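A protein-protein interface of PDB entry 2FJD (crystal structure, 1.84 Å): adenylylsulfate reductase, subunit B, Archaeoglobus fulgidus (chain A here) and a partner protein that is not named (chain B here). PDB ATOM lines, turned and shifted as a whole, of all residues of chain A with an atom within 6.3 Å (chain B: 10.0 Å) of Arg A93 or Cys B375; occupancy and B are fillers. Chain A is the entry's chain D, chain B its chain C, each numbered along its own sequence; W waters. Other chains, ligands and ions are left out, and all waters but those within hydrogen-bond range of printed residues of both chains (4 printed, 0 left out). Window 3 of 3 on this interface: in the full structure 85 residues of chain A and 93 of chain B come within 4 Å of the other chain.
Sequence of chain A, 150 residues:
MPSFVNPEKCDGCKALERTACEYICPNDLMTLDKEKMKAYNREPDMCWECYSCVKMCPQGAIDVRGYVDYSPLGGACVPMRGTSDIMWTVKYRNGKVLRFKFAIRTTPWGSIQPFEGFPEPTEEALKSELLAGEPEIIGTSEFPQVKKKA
SG of Cys B375 sits at hydrogen-bond distance from O of Leu B371.
O of Trp B373 lies within hydrogen-bond range of N of Ile B378 (2.8 Å).
The backbone carbonyl oxygen (O) of Leu A73 is in hydrogen-bond range of the guanidinium group (NH1) of Arg A93 (2.6 Å).
The backbone carbonyl oxygen (O) of Ala A76 sits at hydrogen-bond distance from the backbone NH (N) of Lys A91, 2.8 Å away.
The side-chain amide oxygen (OD1) of Asn A94 is in hydrogen-bond range of the backbone NH (N) of Lys A96, at 2.9 Å.
Printed residues of chain B that touch a printed residue of chain A: Phe B359, Leu B371, Leu B372, Trp B373, Ala B374, Cys B375, Gln B376, Asn B377, Ile B378 and Asp B379.
Hydrophobic or aromatic side chains of chain B within 4 Å of the printed part of chain A: Phe B359, Leu B371, Leu B372 and Ala B374.
Of the 14 printed residues of chain A, 10 touch a printed residue of chain B.
Printed residues of chain A that touch a printed residue of chain B: Gly A66, Tyr A70, Pro A72, Gly A75, Ala A76, Lys A91, Tyr A92, Arg A93, Asn A94 and Lys A96.
Among the printed residues, 20 pairs touch across the chains.
Among the printed residues, Asp or Glu carboxylates within 4 Å of a Lys or Arg side-chain nitrogen of the other chain: Lys A96 with Asp B379 (2.8 Å).
Water W2 lies within hydrogen-bond range of the side-chain hydroxyl of Ser A71 and the backbone NH of Leu B372.
Water W1 lies within hydrogen-bond range of OD1 of Asp B379 and NZ of Lys A96.
Water W4 lies within hydrogen-bond range of O of Gly A75 (2.8 Å), N of Gly A66 (2.8 Å) and SG of Cys B375 (3.3 Å).
Water W3 bridges the backbone carbonyl oxygen (O) of Pro A72 (3.0 Å) and the side-chain sulfur (SG) of Cys B375 (3.8 Å).
The backbone carbonyl oxygen (O) of Ala B374 lies within hydrogen-bond range of the backbone NH (N) of Arg A93 (2.9 Å).
The side-chain sulfur (SG) of Cys B375 sits close to the backbone carbonyl oxygen (O) of Pro A72, at 3.3 Å.
The side-chain sulfur (SG) of Cys B375 lies close to the backbone NH (N) of Gly A75.
NE2 of Gln B376 sits at hydrogen-bond distance from O of Tyr A70 (3.1 Å).
The side-chain amide oxygen of Asn B377 is in hydrogen-bond range of the backbone NH of Arg A93 (3.3 Å).
OD1 of Asn B377 lies within hydrogen-bond range of N of Asn A94 (2.8 Å).
The backbone carbonyl oxygen (O) of Ile B378 is in hydrogen-bond range of the side-chain hydroxyl (OH) of Tyr A92 (2.7 Å).
NZ of Lys A96 is in salt-bridge range of OD1 of Asp B379, 2.8 Å away.
Cys B375 touches just these residues of chain A: Pro A72, Gly A75 and Arg A93.
No residue of chain B comes within 4 Å of Ser A71.
Of chain B, only Cys B375 and Gln B376 come within 4 Å of Pro A72.
No residue of chain B comes within 4 Å of Gly A74.
Gly A75 touches just these residues of chain B: Leu B371 and Cys B375.
Asn A94 touches one residue of chain B.
Of the printed residues of chain A, Ile B378 touches Tyr A92.
Of the printed residues of chain B, Tyr A70 touches Leu B372 (3.7 Å) and Gln B376 (3.1 Å).
Printed residues of chain B within 4 Å of Lys A91: Ala B374 (3.5 Å).
Of the printed residues of chain B, Lys A96 touches Asp B379.
Of the printed residues of chain A, Phe B359 touches Tyr A92.
The nearest residue of chain B that does not touch Arg A93 is Gln B376 (5.2 Å).
Among the printed residues, merely in contact across the chains: Arg A93 with Cys B375, Tyr A92 with Ala B374, Lys A91 with Ala B374, Ala A76 with Leu B371, Tyr A92 with Asn B377, Gly A66 with Leu B371, Gly A75 with Leu B371, Pro A72 with Gln B376, Tyr A92 with Trp B373, Tyr A70 with Leu B372, Tyr A92 with Phe B359 and Tyr A92 with Asp B379.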
ATOM      1  N   GLY A  66      29.055  -1.663 -22.159  1.00  0.00           N
ATOM      2  CA  GLY A  66      29.054  -0.682 -23.238  1.00  0.00           C
ATOM      3  C   GLY A  66      28.745   0.749 -22.837  1.00  0.00           C
ATOM      4  O   GLY A  66      27.902   0.983 -21.975  1.00  0.00           O
ATOM      5  N   TYR A  70      25.291   5.088 -26.275  1.00  0.00           N
ATOM      6  CA  TYR A  70      24.640   4.361 -27.356  1.00  0.00           C
ATOM      7  C   TYR A  70      24.353   2.892 -27.099  1.00  0.00           C
ATOM      8  O   TYR A  70      23.807   2.210 -27.966  1.00  0.00           O
ATOM      9  CB  TYR A  70      25.498   4.484 -28.622  1.00  0.00           C
ATOM     10  CG  TYR A  70      26.878   3.841 -28.526  1.00  0.00           C
ATOM     11  CD1 TYR A  70      27.026   2.453 -28.502  1.00  0.00           C
ATOM     12  CD2 TYR A  70      28.037   4.622 -28.500  1.00  0.00           C
ATOM     13  CE1 TYR A  70      28.291   1.857 -28.462  1.00  0.00           C
ATOM     14  CE2 TYR A  70      29.310   4.034 -28.460  1.00  0.00           C
ATOM     15  CZ  TYR A  70      29.425   2.652 -28.446  1.00  0.00           C
ATOM     16  OH  TYR A  70      30.672   2.063 -28.438  1.00  0.00           O
ATOM     17  N   SER A  71      24.697   2.404 -25.913  1.00  0.00           N
ATOM     18  CA  SER A  71      24.501   0.995 -25.613  1.00  0.00           C
ATOM     19  C   SER A  71      23.311   0.617 -24.751  1.00  0.00           C
ATOM     20  O   SER A  71      23.228   1.014 -23.587  1.00  0.00           O
ATOM     21  CB  SER A  71      25.758   0.426 -24.943  1.00  0.00           C
ATOM     22  OG  SER A  71      26.926   0.748 -25.669  1.00  0.00           O
ATOM     23  N   PRO A  72      22.354  -0.129 -25.321  1.00  0.00           N
ATOM     24  CA  PRO A  72      21.217  -0.523 -24.486  1.00  0.00           C
ATOM     25  C   PRO A  72      21.818  -1.540 -23.515  1.00  0.00           C
ATOM     26  O   PRO A  72      22.859  -2.134 -23.806  1.00  0.00           O
ATOM     27  CB  PRO A  72      20.269  -1.184 -25.487  1.00  0.00           C
ATOM     28  CG  PRO A  72      20.549  -0.442 -26.757  1.00  0.00           C
ATOM     29  CD  PRO A  72      22.059  -0.352 -26.748  1.00  0.00           C
ATOM     30  N   LEU A  73      21.192  -1.742 -22.366  1.00  0.00           N
ATOM     31  CA  LEU A  73      21.712  -2.705 -21.403  1.00  0.00           C
ATOM     32  C   LEU A  73      21.566  -4.136 -21.927  1.00  0.00           C
ATOM     33  O   LEU A  73      20.776  -4.392 -22.840  1.00  0.00           O
ATOM     34  CB  LEU A  73      20.955  -2.576 -20.078  1.00  0.00           C
ATOM     35  CG  LEU A  73      21.075  -1.236 -19.347  1.00  0.00           C
ATOM     36  CD1 LEU A  73      20.124  -1.209 -18.157  1.00  0.00           C
ATOM     37  CD2 LEU A  73      22.513  -1.028 -18.893  1.00  0.00           C
ATOM     38  N   GLY A  74      22.349  -5.061 -21.374  1.00  0.00           N
ATOM     39  CA  GLY A  74      22.219  -6.454 -21.768  1.00  0.00           C
ATOM     40  C   GLY A  74      23.288  -7.156 -22.584  1.00  0.00           C
ATOM     41  O   GLY A  74      23.421  -8.376 -22.491  1.00  0.00           O
ATOM     42  N   GLY A  75      24.042  -6.416 -23.387  1.00  0.00           N
ATOM     43  CA  GLY A  75      25.063  -7.049 -24.204  1.00  0.00           C
ATOM     44  C   GLY A  75      26.390  -7.277 -23.511  1.00  0.00           C
ATOM     45  O   GLY A  75      26.736  -6.575 -22.562  1.00  0.00           O
ATOM     46  N   ALA A  76      27.138  -8.267 -23.983  1.00  0.00           N
ATOM     47  CA  ALA A  76      28.438  -8.553 -23.400  1.00  0.00           C
ATOM     48  C   ALA A  76      29.325  -9.396 -24.308  1.00  0.00           C
ATOM     49  O   ALA A  76      28.845 -10.228 -25.085  1.00  0.00           O
ATOM     50  CB  ALA A  76      28.267  -9.244 -22.045  1.00  0.00           C
ATOM     51  N   LYS A  91      27.192 -12.314 -26.022  1.00  0.00           N
ATOM     52  CA  LYS A  91      25.827 -12.455 -25.542  1.00  0.00           C
ATOM     53  C   LYS A  91      24.999 -11.230 -25.883  1.00  0.00           C
ATOM     54  O   LYS A  91      25.306 -10.113 -25.461  1.00  0.00           O
ATOM     55  CB  LYS A  91      25.811 -12.693 -24.031  1.00  0.00           C
ATOM     56  CG  LYS A  91      24.420 -13.011 -23.484  1.00  0.00           C
ATOM     57  CD  LYS A  91      24.489 -13.573 -22.072  1.00  0.00           C
ATOM     58  CE  LYS A  91      23.148 -14.160 -21.650  1.00  0.00           C
ATOM     59  NZ  LYS A  91      23.217 -14.820 -20.310  1.00  0.00           N
ATOM     60  N   TYR A  92      23.942 -11.461 -26.650  1.00  0.00           N
ATOM     61  CA  TYR A  92      23.038 -10.410 -27.078  1.00  0.00           C
ATOM     62  C   TYR A  92      22.049 -10.012 -25.995  1.00  0.00           C
ATOM     63  O   TYR A  92      21.756 -10.787 -25.083  1.00  0.00           O
ATOM     64  CB  TYR A  92      22.260 -10.876 -28.309  1.00  0.00           C
ATOM     65  CG  TYR A  92      22.997 -10.690 -29.611  1.00  0.00           C
ATOM     66  CD1 TYR A  92      24.309 -11.139 -29.765  1.00  0.00           C
ATOM     67  CD2 TYR A  92      22.390 -10.047 -30.685  1.00  0.00           C
ATOM     68  CE1 TYR A  92      24.998 -10.942 -30.963  1.00  0.00           C
ATOM     69  CE2 TYR A  92      23.065  -9.849 -31.882  1.00  0.00           C
ATOM     70  CZ  TYR A  92      24.368 -10.296 -32.015  1.00  0.00           C
ATOM     71  OH  TYR A  92      25.040 -10.075 -33.196  1.00  0.00           O
ATOM     72  N   ARG A  93      21.535  -8.793 -26.111  1.00  0.00           N
ATOM     73  CA  ARG A  93      20.544  -8.282 -25.175  1.00  0.00           C
ATOM     74  C   ARG A  93      19.344  -9.230 -25.187  1.00  0.00           C
ATOM     75  O   ARG A  93      18.739  -9.485 -24.145  1.00  0.00           O
ATOM     76  CB  ARG A  93      20.114  -6.876 -25.610  1.00  0.00           C
ATOM     77  CG  ARG A  93      18.961  -6.242 -24.830  1.00  0.00           C
ATOM     78  CD  ARG A  93      18.578  -4.930 -25.522  1.00  0.00           C
ATOM     79  NE  ARG A  93      17.372  -4.287 -25.004  1.00  0.00           N
ATOM     80  CZ  ARG A  93      17.325  -3.502 -23.930  1.00  0.00           C
ATOM     81  NH1 ARG A  93      18.422  -3.251 -23.223  1.00  0.00           N
ATOM     82  NH2 ARG A  93      16.178  -2.938 -23.580  1.00  0.00           N
ATOM     83  N   ASN A  94      19.009  -9.758 -26.364  1.00  0.00           N
ATOM     84  CA  ASN A  94      17.869 -10.668 -26.480  1.00  0.00           C
ATOM     85  C   ASN A  94      18.149 -12.099 -26.012  1.00  0.00           C
ATOM     86  O   ASN A  94      17.272 -12.963 -26.090  1.00  0.00           O
ATOM     87  CB  ASN A  94      17.325 -10.697 -27.916  1.00  0.00           C
ATOM     88  CG  ASN A  94      18.320 -11.253 -28.922  1.00  0.00           C
ATOM     89  OD1 ASN A  94      19.189 -12.053 -28.585  1.00  0.00           O
ATOM     90  ND2 ASN A  94      18.174 -10.843 -30.178  1.00  0.00           N
ATOM     91  N   GLY A  95      19.364 -12.350 -25.533  1.00  0.00           N
ATOM     92  CA  GLY A  95      19.695 -13.678 -25.045  1.00  0.00           C
ATOM     93  C   GLY A  95      20.502 -14.567 -25.973  1.00  0.00           C
ATOM     94  O   GLY A  95      21.051 -15.578 -25.532  1.00  0.00           O
ATOM     95  N   LYS A  96      20.567 -14.210 -27.251  1.00  0.00           N
ATOM     96  CA  LYS A  96      21.332 -14.994 -28.211  1.00  0.00           C
ATOM     97  C   LYS A  96      22.771 -15.091 -27.722  1.00  0.00           C
ATOM     98  O   LYS A  96      23.314 -14.128 -27.184  1.00  0.00           O
ATOM     99  CB  LYS A  96      21.294 -14.325 -29.583  1.00  0.00           C
ATOM    100  CG  LYS A  96      22.102 -15.036 -30.654  1.00  0.00           C
ATOM    101  CD  LYS A  96      21.935 -14.350 -31.998  1.00  0.00           C
ATOM    102  CE  LYS A  96      22.576 -15.160 -33.108  1.00  0.00           C
ATOM    103  NZ  LYS A  96      22.312 -14.556 -34.437  1.00  0.00           N
ATOM    104  N   PHE B 359      33.024 -11.833 -37.578  1.00  0.00           N
ATOM    105  CA  PHE B 359      33.130 -11.503 -36.166  1.00  0.00           C
ATOM    106  C   PHE B 359      34.573 -11.389 -35.693  1.00  0.00           C
ATOM    107  O   PHE B 359      34.874 -10.561 -34.834  1.00  0.00           O
ATOM    108  CB  PHE B 359      32.351 -12.498 -35.298  1.00  0.00           C
ATOM    109  CG  PHE B 359      30.930 -12.074 -35.043  1.00  0.00           C
ATOM    110  CD1 PHE B 359      29.942 -12.284 -35.996  1.00  0.00           C
ATOM    111  CD2 PHE B 359      30.596 -11.405 -33.872  1.00  0.00           C
ATOM    112  CE1 PHE B 359      28.642 -11.828 -35.788  1.00  0.00           C
ATOM    113  CE2 PHE B 359      29.298 -10.947 -33.655  1.00  0.00           C
ATOM    114  CZ  PHE B 359      28.321 -11.158 -34.615  1.00  0.00           C
ATOM    115  N   VAL B 367      36.502  -4.456 -30.250  1.00  0.00           N
ATOM    116  CA  VAL B 367      35.473  -5.226 -29.570  1.00  0.00           C
ATOM    117  C   VAL B 367      34.193  -4.431 -29.354  1.00  0.00           C
ATOM    118  O   VAL B 367      33.100  -4.996 -29.377  1.00  0.00           O
ATOM    119  CB  VAL B 367      35.989  -5.746 -28.211  1.00  0.00           C
ATOM    120  CG1 VAL B 367      35.001  -6.737 -27.624  1.00  0.00           C
ATOM    121  CG2 VAL B 367      37.357  -6.404 -28.391  1.00  0.00           C
ATOM    122  N   SER B 368      34.328  -3.121 -29.155  1.00  0.00           N
ATOM    123  CA  SER B 368      33.168  -2.262 -28.939  1.00  0.00           C
ATOM    124  C   SER B 368      32.106  -2.416 -30.015  1.00  0.00           C
ATOM    125  O   SER B 368      30.917  -2.278 -29.735  1.00  0.00           O
ATOM    126  CB  SER B 368      33.582  -0.784 -28.864  1.00  0.00           C
ATOM    127  OG  SER B 368      34.235  -0.484 -27.641  1.00  0.00           O
ATOM    128  N   GLN B 369      32.517  -2.687 -31.251  1.00  0.00           N
ATOM    129  CA  GLN B 369      31.529  -2.828 -32.310  1.00  0.00           C
ATOM    130  C   GLN B 369      30.751  -4.127 -32.153  1.00  0.00           C
ATOM    131  O   GLN B 369      29.550  -4.170 -32.408  1.00  0.00           O
ATOM    132  CB  GLN B 369      32.177  -2.776 -33.696  1.00  0.00           C
ATOM    133  CG  GLN B 369      31.152  -2.712 -34.826  1.00  0.00           C
ATOM    134  CD  GLN B 369      30.279  -1.467 -34.770  1.00  0.00           C
ATOM    135  OE1 GLN B 369      29.061  -1.532 -34.970  1.00  0.00           O
ATOM    136  NE2 GLN B 369      30.898  -0.323 -34.516  1.00  0.00           N
ATOM    137  N   ALA B 370      31.432  -5.192 -31.739  1.00  0.00           N
ATOM    138  CA  ALA B 370      30.744  -6.465 -31.540  1.00  0.00           C
ATOM    139  C   ALA B 370      29.816  -6.285 -30.345  1.00  0.00           C
ATOM    140  O   ALA B 370      28.706  -6.814 -30.321  1.00  0.00           O
ATOM    141  CB  ALA B 370      31.747  -7.586 -31.271  1.00  0.00           C
ATOM    142  N   LEU B 371      30.277  -5.525 -29.355  1.00  0.00           N
ATOM    143  CA  LEU B 371      29.481  -5.264 -28.163  1.00  0.00           C
ATOM    144  C   LEU B 371      28.265  -4.414 -28.523  1.00  0.00           C
ATOM    145  O   LEU B 371      27.171  -4.627 -28.005  1.00  0.00           O
ATOM    146  CB  LEU B 371      30.326  -4.544 -27.107  1.00  0.00           C
ATOM    147  CG  LEU B 371      29.640  -4.257 -25.767  1.00  0.00           C
ATOM    148  CD1 LEU B 371      29.161  -5.565 -25.147  1.00  0.00           C
ATOM    149  CD2 LEU B 371      30.618  -3.549 -24.832  1.00  0.00           C
ATOM    150  N   LEU B 372      28.457  -3.455 -29.423  1.00  0.00           N
ATOM    151  CA  LEU B 372      27.356  -2.595 -29.847  1.00  0.00           C
ATOM    152  C   LEU B 372      26.286  -3.464 -30.502  1.00  0.00           C
ATOM    153  O   LEU B 372      25.100  -3.349 -30.180  1.00  0.00           O
ATOM    154  CB  LEU B 372      27.864  -1.527 -30.824  1.00  0.00           C
ATOM    155  CG  LEU B 372      26.878  -0.475 -31.357  1.00  0.00           C
ATOM    156  CD1 LEU B 372      27.661   0.696 -31.947  1.00  0.00           C
ATOM    157  CD2 LEU B 372      25.968  -1.090 -32.416  1.00  0.00           C
ATOM    158  N   TRP B 373      26.709  -4.336 -31.415  1.00  0.00           N
ATOM    159  CA  TRP B 373      25.785  -5.239 -32.099  1.00  0.00           C
ATOM    160  C   TRP B 373      25.000  -6.084 -31.098  1.00  0.00           C
ATOM    161  O   TRP B 373      23.789  -6.267 -31.235  1.00  0.00           O
ATOM    162  CB  TRP B 373      26.547  -6.177 -33.044  1.00  0.00           C
ATOM    163  CG  TRP B 373      26.870  -5.590 -34.387  1.00  0.00           C
ATOM    164  CD1 TRP B 373      26.499  -4.364 -34.866  1.00  0.00           C
ATOM    165  CD2 TRP B 373      27.576  -6.241 -35.452  1.00  0.00           C
ATOM    166  NE1 TRP B 373      26.927  -4.216 -36.167  1.00  0.00           N
ATOM    167  CE2 TRP B 373      27.589  -5.352 -36.550  1.00  0.00           C
ATOM    168  CE3 TRP B 373      28.195  -7.491 -35.586  1.00  0.00           C
ATOM    169  CZ2 TRP B 373      28.200  -5.675 -37.768  1.00  0.00           C
ATOM    170  CZ3 TRP B 373      28.802  -7.812 -36.798  1.00  0.00           C
ATOM    171  CH2 TRP B 373      28.799  -6.907 -37.872  1.00  0.00           C
ATOM    172  N   ALA B 374      25.699  -6.600 -30.093  1.00  0.00           N
ATOM    173  CA  ALA B 374      25.068  -7.425 -29.072  1.00  0.00           C
ATOM    174  C   ALA B 374      24.036  -6.631 -28.272  1.00  0.00           C
ATOM    175  O   ALA B 374      22.920  -7.106 -28.044  1.00  0.00           O
ATOM    176  CB  ALA B 374      26.129  -8.004 -28.138  1.00  0.00           C
ATOM    177  N   CYS B 375      24.407  -5.427 -27.846  1.00  0.00           N
ATOM    178  CA  CYS B 375      23.506  -4.580 -27.068  1.00  0.00           C
ATOM    179  C   CYS B 375      22.288  -4.120 -27.864  1.00  0.00           C
ATOM    180  O   CYS B 375      21.210  -3.935 -27.297  1.00  0.00           O
ATOM    181  CB  CYS B 375      24.245  -3.343 -26.545  1.00  0.00           C
ATOM    182  SG  CYS B 375      25.462  -3.659 -25.258  1.00  0.00           S
ATOM    183  N   GLN B 376      22.467  -3.932 -29.170  1.00  0.00           N
ATOM    184  CA  GLN B 376      21.387  -3.474 -30.036  1.00  0.00           C
ATOM    185  C   GLN B 376      20.699  -4.597 -30.810  1.00  0.00           C
ATOM    186  O   GLN B 376      19.871  -4.340 -31.686  1.00  0.00           O
ATOM    187  CB  GLN B 376      21.922  -2.420 -31.008  1.00  0.00           C
ATOM    188  CG  GLN B 376      22.145  -1.057 -30.355  1.00  0.00           C
ATOM    189  CD  GLN B 376      22.821  -0.060 -31.273  1.00  0.00           C
ATOM    190  OE1 GLN B 376      22.629  -0.087 -32.483  1.00  0.00           O
ATOM    191  NE2 GLN B 376      23.608   0.836 -30.694  1.00  0.00           N
ATOM    192  N   ASN B 377      21.040  -5.838 -30.471  1.00  0.00           N
ATOM    193  CA  ASN B 377      20.467  -7.012 -31.123  1.00  0.00           C
ATOM    194  C   ASN B 377      20.599  -6.995 -32.638  1.00  0.00           C
ATOM    195  O   ASN B 377      19.655  -7.315 -33.361  1.00  0.00           O
ATOM    196  CB  ASN B 377      18.997  -7.167 -30.734  1.00  0.00           C
ATOM    197  CG  ASN B 377      18.828  -7.577 -29.289  1.00  0.00           C
ATOM    198  OD1 ASN B 377      19.622  -8.361 -28.766  1.00  0.00           O
ATOM    199  ND2 ASN B 377      17.790  -7.063 -28.638  1.00  0.00           N
ATOM    200  N   ILE B 378      21.777  -6.626 -33.119  1.00  0.00           N
ATOM    201  CA  ILE B 378      22.017  -6.582 -34.550  1.00  0.00           C
ATOM    202  C   ILE B 378      22.780  -7.823 -35.007  1.00  0.00           C
ATOM    203  O   ILE B 378      23.900  -8.077 -34.561  1.00  0.00           O
ATOM    204  CB  ILE B 378      22.826  -5.316 -34.946  1.00  0.00           C
ATOM    205  CG1 ILE B 378      21.998  -4.058 -34.664  1.00  0.00           C
ATOM    206  CG2 ILE B 378      23.215  -5.374 -36.426  1.00  0.00           C
ATOM    207  CD1 ILE B 378      22.776  -2.764 -34.850  1.00  0.00           C
ATOM    208  N   ASP B 379      22.149  -8.609 -35.873  1.00  0.00           N
ATOM    209  CA  ASP B 379      22.774  -9.801 -36.432  1.00  0.00           C
ATOM    210  C   ASP B 379      23.118  -9.405 -37.863  1.00  0.00           C
ATOM    211  O   ASP B 379      22.227  -9.206 -38.685  1.00  0.00           O
ATOM    212  CB  ASP B 379      21.798 -10.980 -36.426  1.00  0.00           C
ATOM    213  CG  ASP B 379      22.406 -12.245 -37.001  1.00  0.00           C
ATOM    214  OD1 ASP B 379      21.787 -13.322 -36.854  1.00  0.00           O
ATOM    215  OD2 ASP B 379      23.499 -12.168 -37.603  1.00  0.00           O
HETATM  216  O   HOH W   1      19.284 -13.522 -35.648  1.00  0.00           O
HETATM  217  O   HOH W   2      28.095  -1.351 -26.953  1.00  0.00           O
HETATM  218  O   HOH W   3      25.024  -2.230 -21.766  1.00  0.00           O
HETATM  219  O   HOH W   4      27.240  -3.819 -22.428  1.00  0.00           O
